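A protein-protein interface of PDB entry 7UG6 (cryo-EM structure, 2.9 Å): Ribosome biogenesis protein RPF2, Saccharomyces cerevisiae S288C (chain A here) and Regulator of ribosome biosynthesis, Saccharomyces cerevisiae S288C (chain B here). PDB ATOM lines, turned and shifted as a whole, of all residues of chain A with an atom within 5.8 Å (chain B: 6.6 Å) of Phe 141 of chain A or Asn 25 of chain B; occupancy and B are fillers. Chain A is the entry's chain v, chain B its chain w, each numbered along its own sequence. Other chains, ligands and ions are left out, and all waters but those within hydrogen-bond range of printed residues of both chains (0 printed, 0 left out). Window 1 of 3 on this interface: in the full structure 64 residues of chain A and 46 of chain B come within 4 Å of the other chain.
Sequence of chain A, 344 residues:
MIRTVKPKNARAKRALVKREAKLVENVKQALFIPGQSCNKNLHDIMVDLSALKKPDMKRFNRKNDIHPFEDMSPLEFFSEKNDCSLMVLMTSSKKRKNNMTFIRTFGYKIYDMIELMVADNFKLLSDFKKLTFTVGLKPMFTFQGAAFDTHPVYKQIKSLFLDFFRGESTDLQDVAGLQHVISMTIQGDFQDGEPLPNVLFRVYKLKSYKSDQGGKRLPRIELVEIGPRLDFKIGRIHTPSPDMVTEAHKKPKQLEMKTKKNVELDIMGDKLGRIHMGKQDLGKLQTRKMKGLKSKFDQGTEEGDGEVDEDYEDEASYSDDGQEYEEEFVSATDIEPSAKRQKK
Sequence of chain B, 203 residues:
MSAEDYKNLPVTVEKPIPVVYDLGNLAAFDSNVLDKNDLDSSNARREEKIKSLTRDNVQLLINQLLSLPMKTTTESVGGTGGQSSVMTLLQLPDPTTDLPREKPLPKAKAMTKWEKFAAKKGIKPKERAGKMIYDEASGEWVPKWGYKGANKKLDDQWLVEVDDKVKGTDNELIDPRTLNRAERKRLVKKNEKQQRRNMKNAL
The backbone carbonyl oxygen (O) of Leu 26 of chain B is in hydrogen-bond range of the backbone NH (N) of Phe 141 of chain A (2.7 Å).
O of Phe 141 of chain A is in hydrogen-bond range of N of Ala 28 of chain B, 3.1 Å away.
The side-chain amide oxygen of Asn 25 of chain B lies within hydrogen-bond range of the guanidinium group of Arg 166 of chain A.
The side-chain amino group (NZ) of Lys 138 of chain A lies within hydrogen-bond range of the backbone carbonyl oxygen (O) of Asn 25 of chain B, 3.3 Å away.
The backbone NH (N) of Phe 143 of chain A sits at hydrogen-bond distance from the backbone carbonyl oxygen (O) of Ala 28 of chain B.
Of the 18 printed residues of chain B, 11 touch a printed residue of chain A.
Hydrophobic or aromatic side chains of chain B within 4 Å of the printed part of chain A: Leu 26, Ala 27, Phe 29, Val 58, Leu 61, Pro 95 and Leu 99.
Hydrophobic or aromatic side chains of chain A that line the printed part of chain B: Met 140, Phe 141, Phe 143, Leu 162 and Val 181.
Among the printed residues, no Asp or Glu carboxylate lies within 4 Å of a Lys or Arg side-chain nitrogen of the other chain.
N of Asp 22 of chain B sits at hydrogen-bond distance from O of Ala 27 of chain B (2.8 Å).
The side-chain hydroxyl (OG) of Ser 183 of chain A sits at hydrogen-bond distance from the side-chain hydroxyl (OG1) of Thr 142 of chain A (3.2 Å).
N of Thr 97 of chain B lies within hydrogen-bond range of OD1 of Asp 22 of chain B (3.0 Å).
O of Thr 142 of chain A sits at hydrogen-bond distance from N of Met 184 of chain A, 3.1 Å away.
The backbone NH (N) of Ile 182 of chain A lies within hydrogen-bond range of the backbone carbonyl oxygen (O) of Met 140 of chain A (2.8 Å).
N of Thr 142 of chain A is in hydrogen-bond range of O of Ile 182 of chain A, 3.0 Å away.
Phe 141 of chain A touches just these residues of chain B: Asn 25 (3.5 Å), Leu 26 (2.7 Å), Ala 27 (3.3 Å), Ala 28 (3.1 Å) and Leu 61 (3.6 Å).
Asn 25 of chain B touches just these residues of chain A: Lys 138, Pro 139, Phe 141 and Arg 166.
Of the printed residues of chain B, Arg 166 of chain A touches Asn 25 (2.9 Å) and Leu 99 (3.6 Å).
Of the printed residues of chain A, Asn 57 of chain B touches Thr 142.
Of the printed residues of chain B, Lys 138 of chain A touches Asn 25 and Leu 26.
Printed residues of chain A within 4 Å of Thr 97 of chain B: Leu 162 (3.98 Å).
Of the printed residues of chain A, Ala 28 of chain B touches Phe 141 (3.1 Å), Thr 142 (3.4 Å) and Phe 143 (3.2 Å).
Pro 93 of chain B touches none of the printed residues of chain A.
The nearest residue of chain B that does not touch Phe 141 of chain A is Phe 29 of chain B (5.8 Å).
Among the printed residues, pairs that only touch across the chains: Lys 138 of chain A with Leu 26 of chain B (3.97 Å), Pro 139 of chain A with Asn 25 of chain B (3.9 Å), Met 140 of chain A with Leu 26 of chain B (3.2 Å), Met 140 of chain A with Val 58 of chain B (3.7 Å), Met 140 of chain A with Leu 61 of chain B (3.5 Å), Phe 141 of chain A with Asn 25 of chain B (3.5 Å), Phe 141 of chain A with Ala 27 of chain B (3.3 Å), Phe 141 of chain A with Leu 61 of chain B (3.6 Å), Thr 142 of chain A with Ala 28 of chain B (3.4 Å), Thr 142 of chain A with Asn 57 of chain B (3.9 Å), Thr 142 of chain A with Val 58 of chain B (3.8 Å), Phe 143 of chain A with Phe 29 of chain B (3.6 Å), Leu 162 of chain A with Phe 29 of chain B (3.9 Å), Leu 162 of chain A with Thr 97 of chain B (3.98 Å), Arg 166 of chain A with Leu 99 of chain B (3.6 Å), Ser 169 of chain A with Pro 95 of chain B (3.96 Å) and Val 181 of chain A with Val 58 of chain B (3.5 Å).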
ATOM      1  N   LYS A 138     -13.755 -18.065  -3.200  1.00  0.00           N
ATOM      2  CA  LYS A 138     -13.300 -18.803  -2.030  1.00  0.00           C
ATOM      3  C   LYS A 138     -12.654 -17.849  -1.039  1.00  0.00           C
ATOM      4  O   LYS A 138     -11.678 -17.183  -1.389  1.00  0.00           O
ATOM      5  CB  LYS A 138     -12.295 -19.859  -2.448  1.00  0.00           C
ATOM      6  CG  LYS A 138     -11.641 -20.648  -1.337  1.00  0.00           C
ATOM      7  CD  LYS A 138     -12.334 -21.962  -1.110  1.00  0.00           C
ATOM      8  CE  LYS A 138     -11.474 -22.888  -0.294  1.00  0.00           C
ATOM      9  NZ  LYS A 138     -11.277 -22.354   1.070  1.00  0.00           N
ATOM     10  N   PRO A 139     -13.148 -17.753   0.186  1.00  0.00           N
ATOM     11  CA  PRO A 139     -12.529 -16.861   1.159  1.00  0.00           C
ATOM     12  C   PRO A 139     -11.489 -17.551   2.011  1.00  0.00           C
ATOM     13  O   PRO A 139     -11.552 -18.744   2.295  1.00  0.00           O
ATOM     14  CB  PRO A 139     -13.713 -16.431   2.028  1.00  0.00           C
ATOM     15  CG  PRO A 139     -14.588 -17.577   2.000  1.00  0.00           C
ATOM     16  CD  PRO A 139     -14.422 -18.281   0.683  1.00  0.00           C
ATOM     17  N   MET A 140     -10.533 -16.753   2.424  1.00  0.00           N
ATOM     18  CA  MET A 140      -9.492 -17.150   3.344  1.00  0.00           C
ATOM     19  C   MET A 140      -9.822 -16.661   4.744  1.00  0.00           C
ATOM     20  O   MET A 140     -10.386 -15.590   4.938  1.00  0.00           O
ATOM     21  CB  MET A 140      -8.156 -16.647   2.808  1.00  0.00           C
ATOM     22  CG  MET A 140      -8.053 -15.159   2.734  1.00  0.00           C
ATOM     23  SD  MET A 140      -6.481 -14.553   2.112  1.00  0.00           S
ATOM     24  CE  MET A 140      -5.420 -14.893   3.499  1.00  0.00           C
ATOM     25  N   PHE A 141      -9.527 -17.497   5.727  1.00  0.00           N
ATOM     26  CA  PHE A 141      -9.993 -17.287   7.087  1.00  0.00           C
ATOM     27  C   PHE A 141      -8.828 -16.951   7.996  1.00  0.00           C
ATOM     28  O   PHE A 141      -7.713 -17.436   7.800  1.00  0.00           O
ATOM     29  CB  PHE A 141     -10.667 -18.515   7.649  1.00  0.00           C
ATOM     30  CG  PHE A 141     -11.883 -18.942   6.917  1.00  0.00           C
ATOM     31  CD1 PHE A 141     -13.127 -18.543   7.336  1.00  0.00           C
ATOM     32  CD2 PHE A 141     -11.791 -19.793   5.842  1.00  0.00           C
ATOM     33  CE1 PHE A 141     -14.248 -18.963   6.677  1.00  0.00           C
ATOM     34  CE2 PHE A 141     -12.908 -20.214   5.183  1.00  0.00           C
ATOM     35  CZ  PHE A 141     -14.135 -19.799   5.595  1.00  0.00           C
ATOM     36  N   THR A 142      -9.094 -16.123   8.996  1.00  0.00           N
ATOM     37  CA  THR A 142      -8.206 -15.957  10.134  1.00  0.00           C
ATOM     38  C   THR A 142      -9.050 -16.057  11.387  1.00  0.00           C
ATOM     39  O   THR A 142     -10.141 -15.486  11.447  1.00  0.00           O
ATOM     40  CB  THR A 142      -7.486 -14.620  10.100  1.00  0.00           C
ATOM     41  OG1 THR A 142      -8.453 -13.580  10.236  1.00  0.00           O
ATOM     42  CG2 THR A 142      -6.739 -14.452   8.810  1.00  0.00           C
ATOM     43  N   PHE A 143      -8.552 -16.780  12.376  1.00  0.00           N
ATOM     44  CA  PHE A 143      -9.244 -16.968  13.641  1.00  0.00           C
ATOM     45  C   PHE A 143      -8.291 -16.581  14.756  1.00  0.00           C
ATOM     46  O   PHE A 143      -7.358 -17.330  15.064  1.00  0.00           O
ATOM     47  CB  PHE A 143      -9.700 -18.412  13.790  1.00  0.00           C
ATOM     48  CG  PHE A 143     -10.798 -18.789  12.864  1.00  0.00           C
ATOM     49  CD1 PHE A 143     -10.526 -19.383  11.666  1.00  0.00           C
ATOM     50  CD2 PHE A 143     -12.106 -18.557  13.198  1.00  0.00           C
ATOM     51  CE1 PHE A 143     -11.536 -19.726  10.818  1.00  0.00           C
ATOM     52  CE2 PHE A 143     -13.108 -18.905  12.351  1.00  0.00           C
ATOM     53  CZ  PHE A 143     -12.825 -19.481  11.163  1.00  0.00           C
ATOM     54  N   PHE A 161     -18.052 -21.763  11.401  1.00  0.00           N
ATOM     55  CA  PHE A 161     -17.837 -20.746  10.390  1.00  0.00           C
ATOM     56  C   PHE A 161     -16.957 -21.252   9.258  1.00  0.00           C
ATOM     57  O   PHE A 161     -17.163 -20.866   8.103  1.00  0.00           O
ATOM     58  CB  PHE A 161     -17.268 -19.501  11.026  1.00  0.00           C
ATOM     59  CG  PHE A 161     -18.315 -18.615  11.621  1.00  0.00           C
ATOM     60  CD1 PHE A 161     -19.336 -18.120  10.838  1.00  0.00           C
ATOM     61  CD2 PHE A 161     -18.265 -18.250  12.947  1.00  0.00           C
ATOM     62  CE1 PHE A 161     -20.297 -17.305  11.372  1.00  0.00           C
ATOM     63  CE2 PHE A 161     -19.215 -17.429  13.478  1.00  0.00           C
ATOM     64  CZ  PHE A 161     -20.237 -16.961  12.692  1.00  0.00           C
ATOM     65  N   LEU A 162     -15.981 -22.114   9.551  1.00  0.00           N
ATOM     66  CA  LEU A 162     -15.249 -22.754   8.461  1.00  0.00           C
ATOM     67  C   LEU A 162     -16.184 -23.550   7.575  1.00  0.00           C
ATOM     68  O   LEU A 162     -16.230 -23.344   6.360  1.00  0.00           O
ATOM     69  CB  LEU A 162     -14.153 -23.665   8.988  1.00  0.00           C
ATOM     70  CG  LEU A 162     -12.840 -23.028   9.367  1.00  0.00           C
ATOM     71  CD1 LEU A 162     -11.973 -24.066  10.013  1.00  0.00           C
ATOM     72  CD2 LEU A 162     -12.207 -22.544   8.111  1.00  0.00           C
ATOM     73  N   PHE A 165     -18.468 -21.118   5.486  1.00  0.00           N
ATOM     74  CA  PHE A 165     -17.976 -20.228   4.447  1.00  0.00           C
ATOM     75  C   PHE A 165     -16.817 -20.781   3.638  1.00  0.00           C
ATOM     76  O   PHE A 165     -16.252 -20.041   2.837  1.00  0.00           O
ATOM     77  CB  PHE A 165     -17.557 -18.896   5.056  1.00  0.00           C
ATOM     78  CG  PHE A 165     -18.691 -18.119   5.641  1.00  0.00           C
ATOM     79  CD1 PHE A 165     -19.626 -17.523   4.828  1.00  0.00           C
ATOM     80  CD2 PHE A 165     -18.817 -17.981   7.006  1.00  0.00           C
ATOM     81  CE1 PHE A 165     -20.654 -16.814   5.359  1.00  0.00           C
ATOM     82  CE2 PHE A 165     -19.853 -17.267   7.538  1.00  0.00           C
ATOM     83  CZ  PHE A 165     -20.771 -16.684   6.707  1.00  0.00           C
ATOM     84  N   ARG A 166     -16.446 -22.051   3.798  1.00  0.00           N
ATOM     85  CA  ARG A 166     -15.303 -22.543   3.040  1.00  0.00           C
ATOM     86  C   ARG A 166     -15.636 -22.765   1.581  1.00  0.00           C
ATOM     87  O   ARG A 166     -14.721 -22.879   0.766  1.00  0.00           O
ATOM     88  CB  ARG A 166     -14.758 -23.836   3.643  1.00  0.00           C
ATOM     89  CG  ARG A 166     -15.733 -24.970   3.638  1.00  0.00           C
ATOM     90  CD  ARG A 166     -15.374 -25.995   4.689  1.00  0.00           C
ATOM     91  NE  ARG A 166     -14.360 -26.943   4.256  1.00  0.00           N
ATOM     92  CZ  ARG A 166     -14.634 -28.149   3.776  1.00  0.00           C
ATOM     93  NH1 ARG A 166     -15.889 -28.549   3.670  1.00  0.00           N
ATOM     94  NH2 ARG A 166     -13.656 -28.956   3.402  1.00  0.00           N
ATOM     95  N   SER A 169     -14.323 -27.184  -1.749  1.00  0.00           N
ATOM     96  CA  SER A 169     -12.955 -27.583  -1.462  1.00  0.00           C
ATOM     97  C   SER A 169     -12.211 -27.828  -2.764  1.00  0.00           C
ATOM     98  O   SER A 169     -12.764 -28.398  -3.708  1.00  0.00           O
ATOM     99  CB  SER A 169     -12.933 -28.836  -0.595  1.00  0.00           C
ATOM    100  OG  SER A 169     -11.614 -29.133  -0.174  1.00  0.00           O
ATOM    101  N   VAL A 181     -10.535 -11.762   2.916  1.00  0.00           N
ATOM    102  CA  VAL A 181     -10.325 -12.567   4.109  1.00  0.00           C
ATOM    103  C   VAL A 181     -11.475 -12.352   5.076  1.00  0.00           C
ATOM    104  O   VAL A 181     -11.970 -11.233   5.234  1.00  0.00           O
ATOM    105  CB  VAL A 181      -8.973 -12.258   4.779  1.00  0.00           C
ATOM    106  CG1 VAL A 181      -8.915 -10.855   5.240  1.00  0.00           C
ATOM    107  CG2 VAL A 181      -8.764 -13.159   5.972  1.00  0.00           C
ATOM    108  N   ILE A 182     -11.923 -13.438   5.693  1.00  0.00           N
ATOM    109  CA  ILE A 182     -12.922 -13.412   6.748  1.00  0.00           C
ATOM    110  C   ILE A 182     -12.211 -13.532   8.082  1.00  0.00           C
ATOM    111  O   ILE A 182     -11.509 -14.520   8.326  1.00  0.00           O
ATOM    112  CB  ILE A 182     -13.921 -14.558   6.581  1.00  0.00           C
ATOM    113  CG1 ILE A 182     -14.803 -14.332   5.371  1.00  0.00           C
ATOM    114  CG2 ILE A 182     -14.748 -14.655   7.781  1.00  0.00           C
ATOM    115  CD1 ILE A 182     -15.718 -15.471   5.112  1.00  0.00           C
ATOM    116  N   SER A 183     -12.392 -12.547   8.953  1.00  0.00           N
ATOM    117  CA  SER A 183     -11.637 -12.463  10.194  1.00  0.00           C
ATOM    118  C   SER A 183     -12.572 -12.544  11.383  1.00  0.00           C
ATOM    119  O   SER A 183     -13.547 -11.796  11.460  1.00  0.00           O
ATOM    120  CB  SER A 183     -10.841 -11.171  10.265  1.00  0.00           C
ATOM    121  OG  SER A 183     -10.088 -11.137  11.459  1.00  0.00           O
ATOM    122  N   MET A 184     -12.254 -13.430  12.321  1.00  0.00           N
ATOM    123  CA  MET A 184     -13.125 -13.729  13.444  1.00  0.00           C
ATOM    124  C   MET A 184     -12.293 -13.765  14.705  1.00  0.00           C
ATOM    125  O   MET A 184     -11.421 -14.624  14.844  1.00  0.00           O
ATOM    126  CB  MET A 184     -13.792 -15.068  13.241  1.00  0.00           C
ATOM    127  CG  MET A 184     -14.725 -15.039  12.095  1.00  0.00           C
ATOM    128  SD  MET A 184     -15.500 -16.607  11.843  1.00  0.00           S
ATOM    129  CE  MET A 184     -16.417 -16.224  10.372  1.00  0.00           C
ATOM    130  N   ASP B  22      -4.145 -24.163   8.120  1.00  0.00           N
ATOM    131  CA  ASP B  22      -4.942 -25.159   7.419  1.00  0.00           C
ATOM    132  C   ASP B  22      -5.052 -24.617   6.004  1.00  0.00           C
ATOM    133  O   ASP B  22      -6.059 -24.013   5.629  1.00  0.00           O
ATOM    134  CB  ASP B  22      -6.286 -25.364   8.072  1.00  0.00           C
ATOM    135  CG  ASP B  22      -7.195 -26.241   7.258  1.00  0.00           C
ATOM    136  OD1 ASP B  22      -6.915 -27.445   7.128  1.00  0.00           O
ATOM    137  OD2 ASP B  22      -8.197 -25.726   6.748  1.00  0.00           O
ATOM    138  N   LEU B  23      -4.008 -24.845   5.215  1.00  0.00           N
ATOM    139  CA  LEU B  23      -3.935 -24.294   3.876  1.00  0.00           C
ATOM    140  C   LEU B  23      -4.977 -24.882   2.948  1.00  0.00           C
ATOM    141  O   LEU B  23      -5.212 -24.325   1.876  1.00  0.00           O
ATOM    142  CB  LEU B  23      -2.545 -24.534   3.307  1.00  0.00           C
ATOM    143  CG  LEU B  23      -1.408 -23.997   4.168  1.00  0.00           C
ATOM    144  CD1 LEU B  23      -0.087 -24.575   3.711  1.00  0.00           C
ATOM    145  CD2 LEU B  23      -1.375 -22.491   4.115  1.00  0.00           C
ATOM    146  N   GLY B  24      -5.594 -25.997   3.329  1.00  0.00           N
ATOM    147  CA  GLY B  24      -6.642 -26.564   2.503  1.00  0.00           C
ATOM    148  C   GLY B  24      -7.875 -25.686   2.454  1.00  0.00           C
ATOM    149  O   GLY B  24      -8.546 -25.595   1.425  1.00  0.00           O
ATOM    150  N   ASN B  25      -8.207 -25.050   3.574  1.00  0.00           N
ATOM    151  CA  ASN B  25      -9.305 -24.100   3.624  1.00  0.00           C
ATOM    152  C   ASN B  25      -8.822 -22.663   3.638  1.00  0.00           C
ATOM    153  O   ASN B  25      -9.629 -21.755   3.845  1.00  0.00           O
ATOM    154  CB  ASN B  25     -10.176 -24.350   4.846  1.00  0.00           C
ATOM    155  CG  ASN B  25     -10.838 -25.689   4.814  1.00  0.00           C
ATOM    156  OD1 ASN B  25     -11.673 -25.960   3.957  1.00  0.00           O
ATOM    157  ND2 ASN B  25     -10.494 -26.532   5.769  1.00  0.00           N
ATOM    158  N   LEU B  26      -7.526 -22.442   3.425  1.00  0.00           N
ATOM    159  CA  LEU B  26      -6.922 -21.114   3.446  1.00  0.00           C
ATOM    160  C   LEU B  26      -7.177 -20.426   4.779  1.00  0.00           C
ATOM    161  O   LEU B  26      -7.662 -19.300   4.835  1.00  0.00           O
ATOM    162  CB  LEU B  26      -7.426 -20.262   2.284  1.00  0.00           C
ATOM    163  CG  LEU B  26      -7.320 -20.899   0.906  1.00  0.00           C
ATOM    164  CD1 LEU B  26      -7.915 -20.000  -0.137  1.00  0.00           C
ATOM    165  CD2 LEU B  26      -5.887 -21.176   0.585  1.00  0.00           C
ATOM    166  N   ALA B  27      -6.859 -21.118   5.862  1.00  0.00           N
ATOM    167  CA  ALA B  27      -7.113 -20.613   7.198  1.00  0.00           C
ATOM    168  C   ALA B  27      -5.830 -20.574   8.007  1.00  0.00           C
ATOM    169  O   ALA B  27      -4.974 -21.449   7.879  1.00  0.00           O
ATOM    170  CB  ALA B  27      -8.138 -21.472   7.928  1.00  0.00           C
ATOM    171  N   ALA B  28      -5.706 -19.554   8.848  1.00  0.00           N
ATOM    172  CA  ALA B  28      -4.624 -19.457   9.813  1.00  0.00           C
ATOM    173  C   ALA B  28      -5.218 -19.182  11.180  1.00  0.00           C
ATOM    174  O   ALA B  28      -5.895 -18.167  11.372  1.00  0.00           O
ATOM    175  CB  ALA B  28      -3.640 -18.355   9.443  1.00  0.00           C
ATOM    176  N   PHE B  29      -4.960 -20.071  12.128  1.00  0.00           N
ATOM    177  CA  PHE B  29      -5.528 -19.963  13.459  1.00  0.00           C
ATOM    178  C   PHE B  29      -4.481 -19.378  14.385  1.00  0.00           C
ATOM    179  O   PHE B  29      -3.431 -19.985  14.606  1.00  0.00           O
ATOM    180  CB  PHE B  29      -6.001 -21.317  13.971  1.00  0.00           C
ATOM    181  CG  PHE B  29      -6.773 -22.089  12.970  1.00  0.00           C
ATOM    182  CD1 PHE B  29      -8.124 -21.886  12.820  1.00  0.00           C
ATOM    183  CD2 PHE B  29      -6.155 -23.038  12.195  1.00  0.00           C
ATOM    184  CE1 PHE B  29      -8.840 -22.598  11.892  1.00  0.00           C
ATOM    185  CE2 PHE B  29      -6.859 -23.756  11.274  1.00  0.00           C
ATOM    186  CZ  PHE B  29      -8.203 -23.537  11.116  1.00  0.00           C
ATOM    187  N   ASN B  57      -2.106 -11.639  10.529  1.00  0.00           N
ATOM    188  CA  ASN B  57      -2.414 -13.043  10.285  1.00  0.00           C
ATOM    189  C   ASN B  57      -2.504 -13.341   8.793  1.00  0.00           C
ATOM    190  O   ASN B  57      -1.973 -14.353   8.326  1.00  0.00           O
ATOM    191  CB  ASN B  57      -3.703 -13.434  10.990  1.00  0.00           C
ATOM    192  CG  ASN B  57      -3.483 -13.762  12.438  1.00  0.00           C
ATOM    193  OD1 ASN B  57      -2.356 -13.971  12.872  1.00  0.00           O
ATOM    194  ND2 ASN B  57      -4.561 -13.814  13.200  1.00  0.00           N
ATOM    195  N   VAL B  58      -3.156 -12.467   8.024  1.00  0.00           N
ATOM    196  CA  VAL B  58      -3.219 -12.645   6.577  1.00  0.00           C
ATOM    197  C   VAL B  58      -1.831 -12.593   5.966  1.00  0.00           C
ATOM    198  O   VAL B  58      -1.542 -13.320   5.015  1.00  0.00           O
ATOM    199  CB  VAL B  58      -4.139 -11.586   5.948  1.00  0.00           C
ATOM    200  CG1 VAL B  58      -4.058 -11.628   4.447  1.00  0.00           C
ATOM    201  CG2 VAL B  58      -5.550 -11.828   6.362  1.00  0.00           C
ATOM    202  N   LEU B  61      -0.292 -15.814   6.473  1.00  0.00           N
ATOM    203  CA  LEU B  61      -0.981 -16.824   5.682  1.00  0.00           C
ATOM    204  C   LEU B  61      -0.517 -16.771   4.240  1.00  0.00           C
ATOM    205  O   LEU B  61      -0.177 -17.799   3.657  1.00  0.00           O
ATOM    206  CB  LEU B  61      -2.495 -16.624   5.740  1.00  0.00           C
ATOM    207  CG  LEU B  61      -3.343 -17.794   5.221  1.00  0.00           C
ATOM    208  CD1 LEU B  61      -4.648 -17.851   5.976  1.00  0.00           C
ATOM    209  CD2 LEU B  61      -3.594 -17.830   3.732  1.00  0.00           C
ATOM    210  N   LEU B  92      -2.780 -26.799  -3.370  1.00  0.00           N
ATOM    211  CA  LEU B  92      -3.123 -26.767  -1.963  1.00  0.00           C
ATOM    212  C   LEU B  92      -3.146 -28.179  -1.405  1.00  0.00           C
ATOM    213  O   LEU B  92      -3.505 -29.115  -2.121  1.00  0.00           O
ATOM    214  CB  LEU B  92      -4.485 -26.128  -1.766  1.00  0.00           C
ATOM    215  CG  LEU B  92      -4.712 -24.707  -2.259  1.00  0.00           C
ATOM    216  CD1 LEU B  92      -6.130 -24.304  -1.971  1.00  0.00           C
ATOM    217  CD2 LEU B  92      -3.758 -23.763  -1.584  1.00  0.00           C
ATOM    218  N   PRO B  93      -2.777 -28.371  -0.149  1.00  0.00           N
ATOM    219  CA  PRO B  93      -2.916 -29.687   0.470  1.00  0.00           C
ATOM    220  C   PRO B  93      -4.359 -29.975   0.848  1.00  0.00           C
ATOM    221  O   PRO B  93      -5.268 -29.179   0.630  1.00  0.00           O
ATOM    222  CB  PRO B  93      -2.020 -29.588   1.702  1.00  0.00           C
ATOM    223  CG  PRO B  93      -1.905 -28.156   1.964  1.00  0.00           C
ATOM    224  CD  PRO B  93      -1.945 -27.474   0.656  1.00  0.00           C
ATOM    225  N   ASP B  94      -4.560 -31.160   1.409  1.00  0.00           N
ATOM    226  CA  ASP B  94      -5.857 -31.503   1.952  1.00  0.00           C
ATOM    227  C   ASP B  94      -6.145 -30.640   3.176  1.00  0.00           C
ATOM    228  O   ASP B  94      -5.222 -30.145   3.824  1.00  0.00           O
ATOM    229  CB  ASP B  94      -5.906 -32.978   2.341  1.00  0.00           C
ATOM    230  CG  ASP B  94      -5.590 -33.901   1.185  1.00  0.00           C
ATOM    231  OD1 ASP B  94      -5.432 -33.403   0.051  1.00  0.00           O
ATOM    232  OD2 ASP B  94      -5.509 -35.126   1.414  1.00  0.00           O
ATOM    233  N   PRO B  95      -7.414 -30.432   3.507  1.00  0.00           N
ATOM    234  CA  PRO B  95      -7.735 -29.652   4.706  1.00  0.00           C
ATOM    235  C   PRO B  95      -7.367 -30.417   5.966  1.00  0.00           C
ATOM    236  O   PRO B  95      -7.882 -31.506   6.228  1.00  0.00           O
ATOM    237  CB  PRO B  95      -9.244 -29.440   4.590  1.00  0.00           C
ATOM    238  CG  PRO B  95      -9.558 -29.701   3.160  1.00  0.00           C
ATOM    239  CD  PRO B  95      -8.613 -30.750   2.728  1.00  0.00           C
ATOM    240  N   THR B  96      -6.451 -29.838   6.745  1.00  0.00           N
ATOM    241  CA  THR B  96      -6.043 -30.452   8.000  1.00  0.00           C
ATOM    242  C   THR B  96      -7.174 -30.481   9.012  1.00  0.00           C
ATOM    243  O   THR B  96      -7.360 -31.494   9.694  1.00  0.00           O
ATOM    244  CB  THR B  96      -4.856 -29.702   8.595  1.00  0.00           C
ATOM    245  OG1 THR B  96      -5.268 -28.382   8.960  1.00  0.00           O
ATOM    246  CG2 THR B  96      -3.732 -29.608   7.580  1.00  0.00           C
ATOM    247  N   THR B  97      -7.936 -29.398   9.122  1.00  0.00           N
ATOM    248  CA  THR B  97      -8.994 -29.326  10.115  1.00  0.00           C
ATOM    249  C   THR B  97     -10.119 -30.276   9.743  1.00  0.00           C
ATOM    250  O   THR B  97     -10.532 -30.350   8.584  1.00  0.00           O
ATOM    251  CB  THR B  97      -9.517 -27.896  10.264  1.00  0.00           C
ATOM    252  OG1 THR B  97     -10.616 -27.884  11.178  1.00  0.00           O
ATOM    253  CG2 THR B  97      -9.959 -27.321   8.939  1.00  0.00           C
ATOM    254  N   LEU B  99     -13.877 -31.443   9.776  1.00  0.00           N
ATOM    255  CA  LEU B  99     -15.169 -30.794   9.792  1.00  0.00           C
ATOM    256  C   LEU B  99     -16.276 -31.809   9.580  1.00  0.00           C
ATOM    257  O   LEU B  99     -16.083 -32.803   8.878  1.00  0.00           O
ATOM    258  CB  LEU B  99     -15.248 -29.718   8.706  1.00  0.00           C
ATOM    259  CG  LEU B  99     -14.838 -28.305   9.101  1.00  0.00           C
ATOM    260  CD1 LEU B  99     -13.403 -28.222   9.506  1.00  0.00           C
ATOM    261  CD2 LEU B  99     -15.055 -27.430   7.922  1.00  0.00           C
